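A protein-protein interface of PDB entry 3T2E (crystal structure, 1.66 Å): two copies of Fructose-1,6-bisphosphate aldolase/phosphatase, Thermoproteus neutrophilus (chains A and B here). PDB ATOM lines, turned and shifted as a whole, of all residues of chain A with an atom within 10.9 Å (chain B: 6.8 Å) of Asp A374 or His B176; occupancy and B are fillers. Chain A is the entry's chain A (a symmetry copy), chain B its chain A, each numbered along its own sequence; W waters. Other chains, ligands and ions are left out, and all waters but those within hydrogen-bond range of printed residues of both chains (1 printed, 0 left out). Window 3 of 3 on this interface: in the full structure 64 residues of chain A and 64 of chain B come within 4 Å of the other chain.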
ATOM      1  N   LYS A 369      18.024  17.141 -10.975  1.00  0.00           N
ATOM      2  CA  LYS A 369      18.332  18.321 -10.193  1.00  0.00           C
ATOM      3  C   LYS A 369      18.819  19.461 -11.078  1.00  0.00           C
ATOM      4  O   LYS A 369      19.792  19.269 -11.836  1.00  0.00           O
ATOM      5  CB  LYS A 369      19.391  17.995  -9.133  1.00  0.00           C
ATOM      6  CG  LYS A 369      19.758  19.228  -8.238  1.00  0.00           C
ATOM      7  CD  LYS A 369      20.480  18.800  -6.940  1.00  0.00           C
ATOM      8  CE  LYS A 369      20.236  19.806  -5.794  1.00  0.00           C
ATOM      9  NZ  LYS A 369      20.620  21.196  -6.132  1.00  0.00           N
ATOM     10  N   PRO A 370      18.174  20.650 -10.998  1.00  0.00           N
ATOM     11  CA  PRO A 370      18.685  21.789 -11.781  1.00  0.00           C
ATOM     12  C   PRO A 370      19.678  22.569 -10.987  1.00  0.00           C
ATOM     13  O   PRO A 370      19.600  22.624  -9.745  1.00  0.00           O
ATOM     14  CB  PRO A 370      17.453  22.678 -11.938  1.00  0.00           C
ATOM     15  CG  PRO A 370      16.755  22.483 -10.529  1.00  0.00           C
ATOM     16  CD  PRO A 370      16.892  20.987 -10.313  1.00  0.00           C
ATOM     17  N   TYR A 371      20.599  23.210 -11.639  1.00  0.00           N
ATOM     18  CA  TYR A 371      21.433  24.135 -10.935  1.00  0.00           C
ATOM     19  C   TYR A 371      21.246  25.447 -11.595  1.00  0.00           C
ATOM     20  O   TYR A 371      21.369  25.545 -12.808  1.00  0.00           O
ATOM     21  CB  TYR A 371      22.899  23.714 -11.001  1.00  0.00           C
ATOM     22  CG  TYR A 371      23.172  22.367 -10.403  1.00  0.00           C
ATOM     23  CD1 TYR A 371      23.509  22.236  -9.046  1.00  0.00           C
ATOM     24  CD2 TYR A 371      23.141  21.189 -11.177  1.00  0.00           C
ATOM     25  CE1 TYR A 371      23.773  20.951  -8.475  1.00  0.00           C
ATOM     26  CE2 TYR A 371      23.377  19.932 -10.632  1.00  0.00           C
ATOM     27  CZ  TYR A 371      23.711  19.815  -9.276  1.00  0.00           C
ATOM     28  OH  TYR A 371      23.956  18.585  -8.757  1.00  0.00           O
ATOM     29  N   PRO A 372      20.959  26.544 -10.821  1.00  0.00           N
ATOM     30  CA  PRO A 372      21.087  27.885 -11.427  1.00  0.00           C
ATOM     31  C   PRO A 372      22.409  28.028 -12.106  1.00  0.00           C
ATOM     32  O   PRO A 372      23.482  27.682 -11.504  1.00  0.00           O
ATOM     33  CB  PRO A 372      20.991  28.879 -10.210  1.00  0.00           C
ATOM     34  CG  PRO A 372      20.283  28.040  -9.181  1.00  0.00           C
ATOM     35  CD  PRO A 372      20.590  26.582  -9.382  1.00  0.00           C
ATOM     36  N   ALA A 373      22.387  28.503 -13.355  1.00  0.00           N
ATOM     37  CA  ALA A 373      23.609  28.465 -14.151  1.00  0.00           C
ATOM     38  C   ALA A 373      24.770  29.301 -13.567  1.00  0.00           C
ATOM     39  O   ALA A 373      25.940  28.922 -13.692  1.00  0.00           O
ATOM     40  CB  ALA A 373      23.347  28.813 -15.574  1.00  0.00           C
ATOM     41  N   ASP A 374      24.426  30.389 -12.867  1.00  0.00           N
ATOM     42  CA  ASP A 374      25.438  31.259 -12.205  1.00  0.00           C
ATOM     43  C   ASP A 374      26.136  30.598 -11.030  1.00  0.00           C
ATOM     44  O   ASP A 374      27.353  30.561 -10.926  1.00  0.00           O
ATOM     45  CB  ASP A 374      24.760  32.568 -11.806  1.00  0.00           C
ATOM     46  CG  ASP A 374      24.592  33.493 -12.997  1.00  0.00           C
ATOM     47  OD1 ASP A 374      25.380  33.376 -13.960  1.00  0.00           O
ATOM     48  OD2 ASP A 374      23.680  34.336 -13.004  1.00  0.00           O
ATOM     49  N   GLN A 375      25.360  29.987 -10.181  1.00  0.00           N
ATOM     50  CA  GLN A 375      25.864  29.256  -9.069  1.00  0.00           C
ATOM     51  C   GLN A 375      26.682  28.080  -9.593  1.00  0.00           C
ATOM     52  O   GLN A 375      27.839  27.905  -9.182  1.00  0.00           O
ATOM     53  CB  GLN A 375      24.682  28.775  -8.259  1.00  0.00           C
ATOM     54  CG  GLN A 375      25.018  28.037  -6.943  1.00  0.00           C
ATOM     55  CD  GLN A 375      23.751  27.631  -6.138  1.00  0.00           C
ATOM     56  OE1 GLN A 375      22.616  27.599  -6.663  1.00  0.00           O
ATOM     57  NE2 GLN A 375      23.955  27.322  -4.852  1.00  0.00           N
ATOM     58  N   TYR A 376      26.088  27.285 -10.516  1.00  0.00           N
ATOM     59  CA  TYR A 376      26.777  26.088 -11.064  1.00  0.00           C
ATOM     60  C   TYR A 376      28.192  26.400 -11.576  1.00  0.00           C
ATOM     61  O   TYR A 376      29.138  25.645 -11.319  1.00  0.00           O
ATOM     62  CB  TYR A 376      25.963  25.440 -12.207  1.00  0.00           C
ATOM     63  CG  TYR A 376      26.732  24.305 -12.863  1.00  0.00           C
ATOM     64  CD1 TYR A 376      26.595  23.041 -12.358  1.00  0.00           C
ATOM     65  CD2 TYR A 376      27.592  24.516 -13.981  1.00  0.00           C
ATOM     66  CE1 TYR A 376      27.295  21.956 -12.887  1.00  0.00           C
ATOM     67  CE2 TYR A 376      28.293  23.423 -14.538  1.00  0.00           C
ATOM     68  CZ  TYR A 376      28.109  22.179 -14.012  1.00  0.00           C
ATOM     69  OH  TYR A 376      28.770  21.082 -14.485  1.00  0.00           O
ATOM     70  N   GLU A 377      28.327  27.485 -12.310  1.00  0.00           N
ATOM     71  CA  GLU A 377      29.603  27.909 -12.873  1.00  0.00           C
ATOM     72  C   GLU A 377      30.773  27.978 -11.827  1.00  0.00           C
ATOM     73  O   GLU A 377      31.902  27.514 -12.088  1.00  0.00           O
ATOM     74  CB  GLU A 377      29.330  29.271 -13.529  1.00  0.00           C
ATOM     75  CG  GLU A 377      30.326  29.717 -14.502  1.00  0.00           C
ATOM     76  CD  GLU A 377      30.578  28.662 -15.549  1.00  0.00           C
ATOM     77  OE1 GLU A 377      29.651  28.311 -16.329  1.00  0.00           O
ATOM     78  OE2 GLU A 377      31.729  28.191 -15.577  1.00  0.00           O
ATOM     79  N   LYS A 378      30.514  28.524 -10.631  1.00  0.00           N
ATOM     80  CA  LYS A 378      31.558  28.511  -9.548  1.00  0.00           C
ATOM     81  C   LYS A 378      31.914  27.132  -9.023  1.00  0.00           C
ATOM     82  O   LYS A 378      33.049  26.882  -8.652  1.00  0.00           O
ATOM     83  CB  LYS A 378      31.138  29.359  -8.343  1.00  0.00           C
ATOM     84  CG  LYS A 378      30.861  30.791  -8.666  1.00  0.00           C
ATOM     85  CD  LYS A 378      30.696  31.594  -7.387  1.00  0.00           C
ATOM     86  CE  LYS A 378      30.309  33.028  -7.744  1.00  0.00           C
ATOM     87  NZ  LYS A 378      31.067  33.982  -6.871  1.00  0.00           N
ATOM     88  N   ASP A 379      30.930  26.264  -8.922  1.00  0.00           N
ATOM     89  CA  ASP A 379      31.112  24.983  -8.259  1.00  0.00           C
ATOM     90  C   ASP A 379      31.142  23.783  -9.227  1.00  0.00           C
ATOM     91  O   ASP A 379      30.947  22.649  -8.781  1.00  0.00           O
ATOM     92  CB  ASP A 379      29.981  24.735  -7.281  1.00  0.00           C
ATOM     93  CG  ASP A 379      29.830  25.865  -6.212  1.00  0.00           C
ATOM     94  OD1 ASP A 379      30.878  26.396  -5.732  1.00  0.00           O
ATOM     95  OD2 ASP A 379      28.643  26.206  -5.906  1.00  0.00           O
ATOM     96  N   ARG A 380      31.351  24.038 -10.531  1.00  0.00           N
ATOM     97  CA  ARG A 380      31.351  22.909 -11.489  1.00  0.00           C
ATOM     98  C   ARG A 380      32.300  21.770 -11.050  1.00  0.00           C
ATOM     99  O   ARG A 380      31.905  20.613 -10.987  1.00  0.00           O
ATOM    100  CB  ARG A 380      31.763  23.383 -12.867  1.00  0.00           C
ATOM    101  CG  ARG A 380      31.998  22.179 -13.854  1.00  0.00           C
ATOM    102  CD  ARG A 380      32.548  22.678 -15.178  1.00  0.00           C
ATOM    103  NE  ARG A 380      31.589  23.364 -16.051  1.00  0.00           N
ATOM    104  CZ  ARG A 380      31.523  24.652 -16.290  1.00  0.00           C
ATOM    105  NH1 ARG A 380      32.349  25.526 -15.654  1.00  0.00           N
ATOM    106  NH2 ARG A 380      30.601  25.115 -17.115  1.00  0.00           N
ATOM    107  N   LYS A 381      33.508  22.132 -10.676  1.00  0.00           N
ATOM    108  CA  LYS A 381      34.497  21.178 -10.206  1.00  0.00           C
ATOM    109  C   LYS A 381      33.986  20.311  -9.066  1.00  0.00           C
ATOM    110  O   LYS A 381      34.173  19.139  -9.057  1.00  0.00           O
ATOM    111  CB  LYS A 381      35.829  21.879  -9.879  1.00  0.00           C
ATOM    112  CG  LYS A 381      35.966  23.296 -10.548  1.00  0.00           C
ATOM    113  CD  LYS A 381      37.408  24.056 -10.463  1.00  0.00           C
ATOM    114  CE  LYS A 381      37.349  25.604 -10.521  1.00  0.00           C
ATOM    115  NZ  LYS A 381      38.183  26.409 -11.573  1.00  0.00           N
ATOM    116  N   TYR A 383      30.766  19.798  -8.283  1.00  0.00           N
ATOM    117  CA  TYR A 383      29.631  18.966  -8.702  1.00  0.00           C
ATOM    118  C   TYR A 383      30.081  17.785  -9.492  1.00  0.00           C
ATOM    119  O   TYR A 383      29.595  16.669  -9.296  1.00  0.00           O
ATOM    120  CB  TYR A 383      28.616  19.787  -9.480  1.00  0.00           C
ATOM    121  CG  TYR A 383      27.947  20.869  -8.677  1.00  0.00           C
ATOM    122  CD1 TYR A 383      27.351  20.602  -7.419  1.00  0.00           C
ATOM    123  CD2 TYR A 383      27.914  22.150  -9.145  1.00  0.00           C
ATOM    124  CE1 TYR A 383      26.743  21.633  -6.688  1.00  0.00           C
ATOM    125  CE2 TYR A 383      27.314  23.201  -8.419  1.00  0.00           C
ATOM    126  CZ  TYR A 383      26.739  22.935  -7.202  1.00  0.00           C
ATOM    127  OH  TYR A 383      26.153  24.004  -6.548  1.00  0.00           O
ATOM    128  N   LEU B 171      22.855  22.754 -20.719  1.00  0.00           N
ATOM    129  CA  LEU B 171      22.435  24.108 -20.388  1.00  0.00           C
ATOM    130  C   LEU B 171      21.038  24.349 -20.950  1.00  0.00           C
ATOM    131  O   LEU B 171      20.829  24.195 -22.166  1.00  0.00           O
ATOM    132  CB  LEU B 171      23.415  25.099 -20.974  1.00  0.00           C
ATOM    133  CG  LEU B 171      23.061  26.580 -20.736  1.00  0.00           C
ATOM    134  CD1 LEU B 171      23.139  26.873 -19.208  1.00  0.00           C
ATOM    135  CD2 LEU B 171      24.126  27.414 -21.412  1.00  0.00           C
ATOM    136  N   ASP B 172      20.087  24.706 -20.088  1.00  0.00           N
ATOM    137  CA  ASP B 172      18.799  25.265 -20.597  1.00  0.00           C
ATOM    138  C   ASP B 172      19.052  26.719 -20.893  1.00  0.00           C
ATOM    139  O   ASP B 172      19.311  27.556 -19.960  1.00  0.00           O
ATOM    140  CB  ASP B 172      17.764  25.076 -19.442  1.00  0.00           C
ATOM    141  CG  ASP B 172      16.433  25.789 -19.726  1.00  0.00           C
ATOM    142  OD1 ASP B 172      16.332  26.593 -20.639  1.00  0.00           O
ATOM    143  OD2 ASP B 172      15.517  25.490 -18.945  1.00  0.00           O
ATOM    144  N   VAL B 173      19.066  27.114 -22.168  1.00  0.00           N
ATOM    145  CA  VAL B 173      19.508  28.436 -22.546  1.00  0.00           C
ATOM    146  C   VAL B 173      18.356  29.477 -22.392  1.00  0.00           C
ATOM    147  O   VAL B 173      18.561  30.670 -22.615  1.00  0.00           O
ATOM    148  CB  VAL B 173      20.005  28.456 -24.003  1.00  0.00           C
ATOM    149  CG1 VAL B 173      21.297  27.546 -24.018  1.00  0.00           C
ATOM    150  CG2 VAL B 173      18.922  27.946 -25.015  1.00  0.00           C
ATOM    151  N   VAL B 174      17.176  28.950 -22.105  1.00  0.00           N
ATOM    152  CA  VAL B 174      15.979  29.812 -21.904  1.00  0.00           C
ATOM    153  C   VAL B 174      15.942  30.245 -20.385  1.00  0.00           C
ATOM    154  O   VAL B 174      15.814  31.477 -20.106  1.00  0.00           O
ATOM    155  CB  VAL B 174      14.679  29.151 -22.333  1.00  0.00           C
ATOM    156  CG1 VAL B 174      13.459  30.048 -21.950  1.00  0.00           C
ATOM    157  CG2 VAL B 174      14.702  28.906 -23.838  1.00  0.00           C
ATOM    158  N   GLU B 175      15.908  29.303 -19.463  1.00  0.00           N
ATOM    159  CA  GLU B 175      15.744  29.623 -18.042  1.00  0.00           C
ATOM    160  C   GLU B 175      17.076  29.666 -17.324  1.00  0.00           C
ATOM    161  O   GLU B 175      17.090  29.923 -16.090  1.00  0.00           O
ATOM    162  CB  GLU B 175      14.879  28.585 -17.391  1.00  0.00           C
ATOM    163  CG  GLU B 175      13.409  28.809 -17.676  1.00  0.00           C
ATOM    164  CD  GLU B 175      12.484  27.728 -17.083  1.00  0.00           C
ATOM    165  OE1 GLU B 175      12.866  26.878 -16.205  1.00  0.00           O
ATOM    166  OE2 GLU B 175      11.342  27.731 -17.548  1.00  0.00           O
ATOM    167  N   HIS B 176      18.190  29.414 -18.031  1.00  0.00           N
ATOM    168  CA  HIS B 176      19.546  29.551 -17.490  1.00  0.00           C
ATOM    169  C   HIS B 176      19.768  28.599 -16.295  1.00  0.00           C
ATOM    170  O   HIS B 176      20.015  29.018 -15.133  1.00  0.00           O
ATOM    171  CB  HIS B 176      19.884  31.057 -17.184  1.00  0.00           C
ATOM    172  CG  HIS B 176      21.361  31.378 -17.162  1.00  0.00           C
ATOM    173  ND1 HIS B 176      22.271  30.881 -18.097  1.00  0.00           N
ATOM    174  CD2 HIS B 176      22.087  32.202 -16.352  1.00  0.00           C
ATOM    175  CE1 HIS B 176      23.481  31.354 -17.842  1.00  0.00           C
ATOM    176  NE2 HIS B 176      23.397  32.154 -16.789  1.00  0.00           N
ATOM    177  N   LYS B 177      19.561  27.294 -16.521  1.00  0.00           N
ATOM    178  CA  LYS B 177      19.638  26.232 -15.499  1.00  0.00           C
ATOM    179  C   LYS B 177      20.546  25.163 -16.133  1.00  0.00           C
ATOM    180  O   LYS B 177      20.513  24.968 -17.378  1.00  0.00           O
ATOM    181  CB  LYS B 177      18.289  25.626 -15.289  1.00  0.00           C
ATOM    182  CG  LYS B 177      17.410  26.662 -14.564  1.00  0.00           C
ATOM    183  CD  LYS B 177      16.008  26.218 -14.458  1.00  0.00           C
ATOM    184  CE  LYS B 177      15.257  27.306 -13.686  1.00  0.00           C
ATOM    185  NZ  LYS B 177      13.816  26.939 -13.637  1.00  0.00           N
ATOM    186  N   VAL B 178      21.317  24.508 -15.301  1.00  0.00           N
ATOM    187  CA  VAL B 178      22.236  23.466 -15.773  1.00  0.00           C
ATOM    188  C   VAL B 178      21.797  22.131 -15.203  1.00  0.00           C
ATOM    189  O   VAL B 178      21.339  21.994 -14.024  1.00  0.00           O
ATOM    190  CB  VAL B 178      23.697  23.772 -15.345  1.00  0.00           C
ATOM    191  CG1 VAL B 178      24.592  22.553 -15.559  1.00  0.00           C
ATOM    192  CG2 VAL B 178      24.176  25.018 -15.960  1.00  0.00           C
ATOM    193  N   ARG B 199      16.669  24.461 -27.009  1.00  0.00           N
ATOM    194  CA  ARG B 199      16.513  24.869 -25.571  1.00  0.00           C
ATOM    195  C   ARG B 199      17.548  24.189 -24.669  1.00  0.00           C
ATOM    196  O   ARG B 199      18.108  24.863 -23.819  1.00  0.00           O
ATOM    197  CB  ARG B 199      15.120  24.527 -25.061  1.00  0.00           C
ATOM    198  CG  ARG B 199      15.059  25.055 -23.607  1.00  0.00           C
ATOM    199  CD  ARG B 199      13.650  25.098 -23.149  1.00  0.00           C
ATOM    200  NE  ARG B 199      13.736  25.506 -21.739  1.00  0.00           N
ATOM    201  CZ  ARG B 199      12.668  25.640 -20.996  1.00  0.00           C
ATOM    202  NH1 ARG B 199      11.483  25.431 -21.576  1.00  0.00           N
ATOM    203  NH2 ARG B 199      12.819  25.989 -19.722  1.00  0.00           N
ATOM    204  N   ARG B 203      26.684  21.272 -23.231  1.00  0.00           N
ATOM    205  CA  ARG B 203      27.726  22.300 -23.236  1.00  0.00           C
ATOM    206  C   ARG B 203      29.111  21.634 -22.952  1.00  0.00           C
ATOM    207  O   ARG B 203      30.115  21.993 -23.528  1.00  0.00           O
ATOM    208  CB  ARG B 203      27.409  23.307 -22.070  1.00  0.00           C
ATOM    209  CG  ARG B 203      28.443  24.406 -22.118  1.00  0.00           C
ATOM    210  CD  ARG B 203      28.019  25.676 -21.264  1.00  0.00           C
ATOM    211  NE  ARG B 203      27.793  25.285 -19.876  1.00  0.00           N
ATOM    212  CZ  ARG B 203      27.318  26.128 -18.928  1.00  0.00           C
ATOM    213  NH1 ARG B 203      27.042  27.405 -19.240  1.00  0.00           N
ATOM    214  NH2 ARG B 203      27.146  25.674 -17.707  1.00  0.00           N
ATOM    215  N   GLU B 220      25.680  29.562 -25.176  1.00  0.00           N
ATOM    216  CA  GLU B 220      25.436  30.576 -24.182  1.00  0.00           C
ATOM    217  C   GLU B 220      23.915  30.718 -24.028  1.00  0.00           C
ATOM    218  O   GLU B 220      23.107  30.431 -24.949  1.00  0.00           O
ATOM    219  CB  GLU B 220      25.966  31.907 -24.677  1.00  0.00           C
ATOM    220  CG  GLU B 220      27.500  31.991 -24.973  1.00  0.00           C
ATOM    221  CD  GLU B 220      28.376  31.594 -23.770  1.00  0.00           C
ATOM    222  OE1 GLU B 220      27.966  31.863 -22.620  1.00  0.00           O
ATOM    223  OE2 GLU B 220      29.513  31.047 -23.982  1.00  0.00           O
ATOM    224  N   ARG B 221      23.525  31.154 -22.818  1.00  0.00           N
ATOM    225  CA  ARG B 221      22.133  31.509 -22.641  1.00  0.00           C
ATOM    226  C   ARG B 221      21.604  32.497 -23.723  1.00  0.00           C
ATOM    227  O   ARG B 221      22.338  33.300 -24.319  1.00  0.00           O
ATOM    228  CB  ARG B 221      22.025  32.068 -21.215  1.00  0.00           C
ATOM    229  CG  ARG B 221      22.501  33.520 -21.114  1.00  0.00           C
ATOM    230  CD  ARG B 221      21.774  34.267 -19.934  1.00  0.00           C
ATOM    231  NE  ARG B 221      20.341  33.916 -19.908  1.00  0.00           N
ATOM    232  CZ  ARG B 221      19.533  33.962 -18.842  1.00  0.00           C
ATOM    233  NH1 ARG B 221      18.267  33.557 -18.959  1.00  0.00           N
ATOM    234  NH2 ARG B 221      19.975  34.398 -17.661  1.00  0.00           N
ATOM    235  N   LEU B 222      20.319  32.432 -24.042  1.00  0.00           N
ATOM    236  CA  LEU B 222      19.752  33.317 -25.081  1.00  0.00           C
ATOM    237  C   LEU B 222      19.514  34.748 -24.545  1.00  0.00           C
ATOM    238  O   LEU B 222      19.179  34.902 -23.337  1.00  0.00           O
ATOM    239  CB  LEU B 222      18.412  32.757 -25.597  1.00  0.00           C
ATOM    240  CG  LEU B 222      18.419  31.398 -26.250  1.00  0.00           C
ATOM    241  CD1 LEU B 222      17.015  30.951 -26.642  1.00  0.00           C
ATOM    242  CD2 LEU B 222      19.317  31.485 -27.510  1.00  0.00           C
HETATM  243  O   HOH W   1      26.910  27.983 -16.140  1.00  0.00           O
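No position is printed for both chains.
Of the 12 pairs that touch across the chains among the printed residues, none has its exchanged pair printed and touching as well.
The backbone NH of Ala A373 sits at hydrogen-bond distance from the backbone carbonyl oxygen of His B176 (3.0 Å).
NH2 of Arg B203 is in salt-bridge range of OE1 of Glu A377.
N of Val B178 lies within hydrogen-bond range of O of Tyr A371 (2.7 Å).
Asp A374 touches one residue of chain B.
Of the printed residues of chain B, Tyr A376 touches Val B178 and Arg B203.
Of the printed residues of chain B, Glu A377 touches Arg B203.
No residue of chain A comes within 4 Å of Asp B172.
No residue of chain A comes within 4 Å of Val B174.
Of the printed residues of chain A, His B176 touches Pro A372 (3.98 Å), Ala A373 (3.0 Å) and Asp A374 (3.7 Å).
Lys B177 touches just one residue of chain A: Tyr A371 (3.3 Å).
The nearest residue of chain B that does not touch Asp A374 is Arg B221 (6.0 Å).
Lys A369 touches Val B178.
Pro A370 touches Val B178.
CA of Lys B177 touches O of Tyr A371, at 3.3 Å.
His B176 touches Pro A372.
Ala A373 touches Val B178.
NE2 of His B176 touches OD1 of Asp A374, 3.7 Å away.
CG1 of Val B178 touches CD1 of Tyr A376 (3.8 Å).
CD2 of Tyr A376 touches NH2 of Arg B203 (3.9 Å).
Arg B203 touches Arg A380.
The side-chain carboxylate (OE2) of Glu A377 lies within salt-bridge range of the guanidinium group (NH1) of Arg A380 (2.7 Å).
NZ of Lys B177 lies within salt-bridge range of OE1 of Glu B175 (2.7 Å).
The backbone NH (N) of Asp B172 sits at hydrogen-bond distance from the backbone carbonyl oxygen (O) of Lys B177, at 2.8 Å.
Among the printed residues, 12 pairs touch across the chains.
Among the printed residues, Asp or Glu carboxylates within 4 Å of a Lys or Arg side-chain nitrogen of the other chain: Glu A377 with Arg B203.
Water W1 lies within hydrogen-bond range of OE1 of Glu A377, O of Ala A373 and NH2 of Arg B203.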
